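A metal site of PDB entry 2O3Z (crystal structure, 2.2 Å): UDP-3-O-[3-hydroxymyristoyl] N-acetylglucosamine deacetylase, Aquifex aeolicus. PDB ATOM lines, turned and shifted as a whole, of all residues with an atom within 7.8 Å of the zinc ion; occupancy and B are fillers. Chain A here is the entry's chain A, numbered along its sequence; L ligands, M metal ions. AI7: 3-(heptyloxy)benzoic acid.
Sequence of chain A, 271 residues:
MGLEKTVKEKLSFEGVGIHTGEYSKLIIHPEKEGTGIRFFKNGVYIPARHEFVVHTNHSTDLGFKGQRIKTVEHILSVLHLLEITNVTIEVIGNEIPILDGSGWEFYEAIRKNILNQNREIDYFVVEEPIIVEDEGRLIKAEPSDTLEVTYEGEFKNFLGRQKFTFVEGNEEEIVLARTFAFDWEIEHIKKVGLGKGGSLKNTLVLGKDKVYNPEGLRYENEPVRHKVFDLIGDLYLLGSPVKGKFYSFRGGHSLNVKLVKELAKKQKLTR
The zinc ion is bound by NE2 of His 226, NE2 of His 74 and OD1 of Asp 230.
Slightly farther from the zinc ion lies OD2 of Asp 230 (2.6 Å).
Within 4 Å of the zinc ion: His 74, His 226 and Asp 230.
The nearest printed residue that does not touch the zinc ion is Glu 73 (4.2 Å).
A ring nitrogen (ND1) of His 226 lies within hydrogen-bond range of the backbone carbonyl oxygen (O) of Ala 177 (2.9 Å).
O of Arg 178 lies within hydrogen-bond range of ND1 of His 226, at 3.3 Å.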
ATOM      1  N   HIS A  58     -34.339  19.481  -7.144  1.00  0.00           N
ATOM      2  CA  HIS A  58     -34.126  18.782  -5.862  1.00  0.00           C
ATOM      3  C   HIS A  58     -32.826  17.988  -5.740  1.00  0.00           C
ATOM      4  O   HIS A  58     -32.540  17.412  -4.691  1.00  0.00           O
ATOM      5  CB  HIS A  58     -35.334  17.907  -5.549  1.00  0.00           C
ATOM      6  CG  HIS A  58     -36.624  18.661  -5.532  1.00  0.00           C
ATOM      7  ND1 HIS A  58     -36.857  19.699  -4.656  1.00  0.00           N
ATOM      8  CD2 HIS A  58     -37.721  18.583  -6.325  1.00  0.00           C
ATOM      9  CE1 HIS A  58     -38.036  20.224  -4.908  1.00  0.00           C
ATOM     10  NE2 HIS A  58     -38.581  19.569  -5.924  1.00  0.00           N
ATOM     11  N   SER A  59     -32.057  17.955  -6.825  1.00  0.00           N
ATOM     12  CA  SER A  59     -30.754  17.287  -6.843  1.00  0.00           C
ATOM     13  C   SER A  59     -30.120  17.461  -8.211  1.00  0.00           C
ATOM     14  O   SER A  59     -30.782  17.898  -9.161  1.00  0.00           O
ATOM     15  CB  SER A  59     -30.869  15.789  -6.481  1.00  0.00           C
ATOM     16  OG  SER A  59     -31.577  15.025  -7.437  1.00  0.00           O
ATOM     17  N   THR A  71     -28.188  12.714  -7.468  1.00  0.00           N
ATOM     18  CA  THR A  71     -27.580  13.396  -6.340  1.00  0.00           C
ATOM     19  C   THR A  71     -26.058  13.320  -6.243  1.00  0.00           C
ATOM     20  O   THR A  71     -25.517  12.787  -5.287  1.00  0.00           O
ATOM     21  CB  THR A  71     -28.220  12.852  -5.048  1.00  0.00           C
ATOM     22  OG1 THR A  71     -29.615  12.635  -5.317  1.00  0.00           O
ATOM     23  CG2 THR A  71     -28.086  13.838  -3.874  1.00  0.00           C
ATOM     24  N   GLU A  73     -24.118  16.129  -6.298  1.00  0.00           N
ATOM     25  CA  GLU A  73     -23.584  17.408  -5.834  1.00  0.00           C
ATOM     26  C   GLU A  73     -22.690  17.384  -4.591  1.00  0.00           C
ATOM     27  O   GLU A  73     -21.700  18.108  -4.542  1.00  0.00           O
ATOM     28  CB  GLU A  73     -24.709  18.427  -5.638  1.00  0.00           C
ATOM     29  CG  GLU A  73     -25.771  18.025  -4.613  1.00  0.00           C
ATOM     30  CD  GLU A  73     -26.983  17.361  -5.243  1.00  0.00           C
ATOM     31  OE1 GLU A  73     -26.809  16.645  -6.239  1.00  0.00           O
ATOM     32  OE2 GLU A  73     -28.113  17.555  -4.719  1.00  0.00           O
ATOM     33  N   HIS A  74     -23.027  16.563  -3.608  1.00  0.00           N
ATOM     34  CA  HIS A  74     -22.252  16.516  -2.373  1.00  0.00           C
ATOM     35  C   HIS A  74     -20.882  15.868  -2.522  1.00  0.00           C
ATOM     36  O   HIS A  74     -19.887  16.388  -2.015  1.00  0.00           O
ATOM     37  CB  HIS A  74     -23.057  15.821  -1.269  1.00  0.00           C
ATOM     38  CG  HIS A  74     -24.350  16.514  -0.964  1.00  0.00           C
ATOM     39  ND1 HIS A  74     -25.318  15.968  -0.142  1.00  0.00           N
ATOM     40  CD2 HIS A  74     -24.843  17.711  -1.386  1.00  0.00           C
ATOM     41  CE1 HIS A  74     -26.343  16.782  -0.083  1.00  0.00           C
ATOM     42  NE2 HIS A  74     -26.092  17.842  -0.823  1.00  0.00           N
ATOM     43  N   ILE A  98     -26.743   9.452   0.693  1.00  0.00           N
ATOM     44  CA  ILE A  98     -26.877  10.780   1.285  1.00  0.00           C
ATOM     45  C   ILE A  98     -26.164  10.862   2.645  1.00  0.00           C
ATOM     46  O   ILE A  98     -25.812  11.953   3.097  1.00  0.00           O
ATOM     47  CB  ILE A  98     -28.365  11.165   1.484  1.00  0.00           C
ATOM     48  CG1 ILE A  98     -28.484  12.619   1.948  1.00  0.00           C
ATOM     49  CG2 ILE A  98     -29.016  10.253   2.528  1.00  0.00           C
ATOM     50  CD1 ILE A  98     -27.960  13.632   0.937  1.00  0.00           C
ATOM     51  N   GLY A 101     -26.347  13.757   5.168  1.00  0.00           N
ATOM     52  CA  GLY A 101     -26.842  14.923   4.450  1.00  0.00           C
ATOM     53  C   GLY A 101     -25.816  16.016   4.193  1.00  0.00           C
ATOM     54  O   GLY A 101     -26.123  17.005   3.524  1.00  0.00           O
ATOM     55  N   SER A 102     -24.608  15.865   4.717  1.00  0.00           N
ATOM     56  CA  SER A 102     -23.557  16.856   4.505  1.00  0.00           C
ATOM     57  C   SER A 102     -22.419  16.170   3.764  1.00  0.00           C
ATOM     58  O   SER A 102     -22.567  15.044   3.285  1.00  0.00           O
ATOM     59  CB  SER A 102     -23.061  17.417   5.839  1.00  0.00           C
ATOM     60  OG  SER A 102     -22.288  16.450   6.543  1.00  0.00           O
ATOM     61  N   ALA A 177     -22.521  21.383   6.989  1.00  0.00           N
ATOM     62  CA  ALA A 177     -23.892  21.870   6.789  1.00  0.00           C
ATOM     63  C   ALA A 177     -24.766  20.806   6.126  1.00  0.00           C
ATOM     64  O   ALA A 177     -24.500  20.395   4.999  1.00  0.00           O
ATOM     65  CB  ALA A 177     -23.882  23.152   5.956  1.00  0.00           C
ATOM     66  N   ARG A 178     -25.825  20.391   6.816  1.00  0.00           N
ATOM     67  CA  ARG A 178     -26.709  19.364   6.288  1.00  0.00           C
ATOM     68  C   ARG A 178     -27.754  19.819   5.267  1.00  0.00           C
ATOM     69  O   ARG A 178     -28.061  21.007   5.153  1.00  0.00           O
ATOM     70  CB  ARG A 178     -27.462  18.668   7.429  1.00  0.00           C
ATOM     71  CG  ARG A 178     -26.558  17.996   8.451  1.00  0.00           C
ATOM     72  CD  ARG A 178     -26.839  18.561   9.834  1.00  0.00           C
ATOM     73  NE  ARG A 178     -28.055  18.023  10.430  1.00  0.00           N
ATOM     74  CZ  ARG A 178     -28.725  18.599  11.417  1.00  0.00           C
ATOM     75  NH1 ARG A 178     -28.296  19.758  11.927  1.00  0.00           N
ATOM     76  NH2 ARG A 178     -29.792  18.009  11.917  1.00  0.00           N
ATOM     77  N   THR A 179     -28.278  18.840   4.548  1.00  0.00           N
ATOM     78  CA  THR A 179     -29.324  19.051   3.555  1.00  0.00           C
ATOM     79  C   THR A 179     -30.523  19.575   4.344  1.00  0.00           C
ATOM     80  O   THR A 179     -30.718  19.197   5.499  1.00  0.00           O
ATOM     81  CB  THR A 179     -29.720  17.691   2.930  1.00  0.00           C
ATOM     82  OG1 THR A 179     -28.646  17.194   2.117  1.00  0.00           O
ATOM     83  CG2 THR A 179     -30.981  17.817   2.113  1.00  0.00           C
ATOM     84  N   PHE A 180     -31.328  20.427   3.727  1.00  0.00           N
ATOM     85  CA  PHE A 180     -32.498  20.947   4.407  1.00  0.00           C
ATOM     86  C   PHE A 180     -33.674  21.081   3.440  1.00  0.00           C
ATOM     87  O   PHE A 180     -33.514  21.032   2.211  1.00  0.00           O
ATOM     88  CB  PHE A 180     -32.190  22.303   5.051  1.00  0.00           C
ATOM     89  CG  PHE A 180     -32.094  23.437   4.075  1.00  0.00           C
ATOM     90  CD1 PHE A 180     -33.206  24.215   3.784  1.00  0.00           C
ATOM     91  CD2 PHE A 180     -30.896  23.709   3.430  1.00  0.00           C
ATOM     92  CE1 PHE A 180     -33.137  25.266   2.857  1.00  0.00           C
ATOM     93  CE2 PHE A 180     -30.804  24.754   2.496  1.00  0.00           C
ATOM     94  CZ  PHE A 180     -31.933  25.531   2.213  1.00  0.00           C
ATOM     95  N   HIS A 226     -25.082  25.291   3.449  1.00  0.00           N
ATOM     96  CA  HIS A 226     -25.295  24.124   2.613  1.00  0.00           C
ATOM     97  C   HIS A 226     -25.480  24.526   1.156  1.00  0.00           C
ATOM     98  O   HIS A 226     -24.991  23.839   0.247  1.00  0.00           O
ATOM     99  CB  HIS A 226     -26.503  23.299   3.073  1.00  0.00           C
ATOM    100  CG  HIS A 226     -26.673  22.037   2.295  1.00  0.00           C
ATOM    101  ND1 HIS A 226     -25.977  20.884   2.596  1.00  0.00           N
ATOM    102  CD2 HIS A 226     -27.358  21.779   1.165  1.00  0.00           C
ATOM    103  CE1 HIS A 226     -26.224  19.981   1.668  1.00  0.00           C
ATOM    104  NE2 HIS A 226     -27.053  20.493   0.783  1.00  0.00           N
ATOM    105  N   LYS A 227     -26.184  25.630   0.920  1.00  0.00           N
ATOM    106  CA  LYS A 227     -26.390  26.102  -0.442  1.00  0.00           C
ATOM    107  C   LYS A 227     -25.041  26.415  -1.102  1.00  0.00           C
ATOM    108  O   LYS A 227     -24.867  26.179  -2.306  1.00  0.00           O
ATOM    109  CB  LYS A 227     -27.278  27.342  -0.436  1.00  0.00           C
ATOM    110  CG  LYS A 227     -28.767  27.034  -0.271  1.00  0.00           C
ATOM    111  CD  LYS A 227     -29.323  26.386  -1.520  1.00  0.00           C
ATOM    112  CE  LYS A 227     -30.836  26.347  -1.515  1.00  0.00           C
ATOM    113  NZ  LYS A 227     -31.367  26.050  -2.881  1.00  0.00           N
ATOM    114  N   PHE A 229     -22.256  24.927  -0.338  1.00  0.00           N
ATOM    115  CA  PHE A 229     -21.697  23.581  -0.539  1.00  0.00           C
ATOM    116  C   PHE A 229     -22.239  22.974  -1.844  1.00  0.00           C
ATOM    117  O   PHE A 229     -21.475  22.417  -2.633  1.00  0.00           O
ATOM    118  CB  PHE A 229     -22.078  22.697   0.665  1.00  0.00           C
ATOM    119  CG  PHE A 229     -21.577  21.297   0.583  1.00  0.00           C
ATOM    120  CD1 PHE A 229     -20.216  21.010   0.679  1.00  0.00           C
ATOM    121  CD2 PHE A 229     -22.469  20.237   0.425  1.00  0.00           C
ATOM    122  CE1 PHE A 229     -19.748  19.693   0.620  1.00  0.00           C
ATOM    123  CE2 PHE A 229     -22.022  18.912   0.363  1.00  0.00           C
ATOM    124  CZ  PHE A 229     -20.647  18.640   0.462  1.00  0.00           C
ATOM    125  N   ASP A 230     -23.551  23.074  -2.072  1.00  0.00           N
ATOM    126  CA  ASP A 230     -24.164  22.542  -3.288  1.00  0.00           C
ATOM    127  C   ASP A 230     -23.624  23.229  -4.540  1.00  0.00           C
ATOM    128  O   ASP A 230     -23.323  22.572  -5.533  1.00  0.00           O
ATOM    129  CB  ASP A 230     -25.694  22.744  -3.284  1.00  0.00           C
ATOM    130  CG  ASP A 230     -26.434  21.701  -2.467  1.00  0.00           C
ATOM    131  OD1 ASP A 230     -25.850  20.650  -2.141  1.00  0.00           O
ATOM    132  OD2 ASP A 230     -27.612  21.921  -2.170  1.00  0.00           O
ATOM    133  N   LEU A 231     -23.504  24.549  -4.503  1.00  0.00           N
ATOM    134  CA  LEU A 231     -23.024  25.310  -5.644  1.00  0.00           C
ATOM    135  C   LEU A 231     -21.591  24.932  -6.013  1.00  0.00           C
ATOM    136  O   LEU A 231     -21.237  24.840  -7.190  1.00  0.00           O
ATOM    137  CB  LEU A 231     -23.128  26.799  -5.338  1.00  0.00           C
ATOM    138  CG  LEU A 231     -22.541  27.806  -6.341  1.00  0.00           C
ATOM    139  CD1 LEU A 231     -22.956  27.440  -7.768  1.00  0.00           C
ATOM    140  CD2 LEU A 231     -23.038  29.209  -5.974  1.00  0.00           C
ATOM    141  N   HIS A 253     -29.905  24.248  -7.887  1.00  0.00           N
ATOM    142  CA  HIS A 253     -29.182  23.453  -8.876  1.00  0.00           C
ATOM    143  C   HIS A 253     -29.448  23.887 -10.321  1.00  0.00           C
ATOM    144  O   HIS A 253     -28.515  24.009 -11.106  1.00  0.00           O
ATOM    145  CB  HIS A 253     -29.525  21.982  -8.725  1.00  0.00           C
ATOM    146  CG  HIS A 253     -29.097  21.407  -7.413  1.00  0.00           C
ATOM    147  ND1 HIS A 253     -27.773  21.369  -7.015  1.00  0.00           N
ATOM    148  CD2 HIS A 253     -29.814  20.871  -6.394  1.00  0.00           C
ATOM    149  CE1 HIS A 253     -27.696  20.844  -5.797  1.00  0.00           C
ATOM    150  NE2 HIS A 253     -28.923  20.529  -5.404  1.00  0.00           N
HETATM  151  C1  AI7 L   1     -39.100  12.573   4.919  1.00  0.00           C
HETATM  152  C2  AI7 L   1     -38.434  13.865   7.338  1.00  0.00           C
HETATM  153  C3  AI7 L   1     -39.158  12.643   7.380  1.00  0.00           C
HETATM  154  C4  AI7 L   1     -34.572  16.993   0.214  1.00  0.00           C
HETATM  155  C5  AI7 L   1     -40.269  10.690   6.188  1.00  0.00           C
HETATM  156  C6  AI7 L   1     -37.103  15.649   1.897  1.00  0.00           C
HETATM  157  C7  AI7 L   1     -38.049  14.420   6.083  1.00  0.00           C
HETATM  158  C8  AI7 L   1     -37.166  15.337   3.389  1.00  0.00           C
HETATM  159  C9  AI7 L   1     -33.313  18.922  -0.835  1.00  0.00           C
HETATM  160  C10 AI7 L   1     -34.174  17.674  -1.098  1.00  0.00           C
HETATM  161  C11 AI7 L   1     -38.363  13.792   4.838  1.00  0.00           C
HETATM  162  C12 AI7 L   1     -35.435  15.743  -0.038  1.00  0.00           C
HETATM  163  C13 AI7 L   1     -35.832  15.048   1.273  1.00  0.00           C
HETATM  164  C14 AI7 L   1     -39.504  11.983   6.158  1.00  0.00           C
HETATM  165  O15 AI7 L   1     -40.651  10.103   7.328  1.00  0.00           O
HETATM  166  O16 AI7 L   1     -38.046  14.247   3.565  1.00  0.00           O
HETATM  167  O17 AI7 L   1     -40.569  10.100   5.150  1.00  0.00           O
HETATM  168 ZN    ZN M   1     -27.264  19.556  -1.035  1.00  0.00          ZN
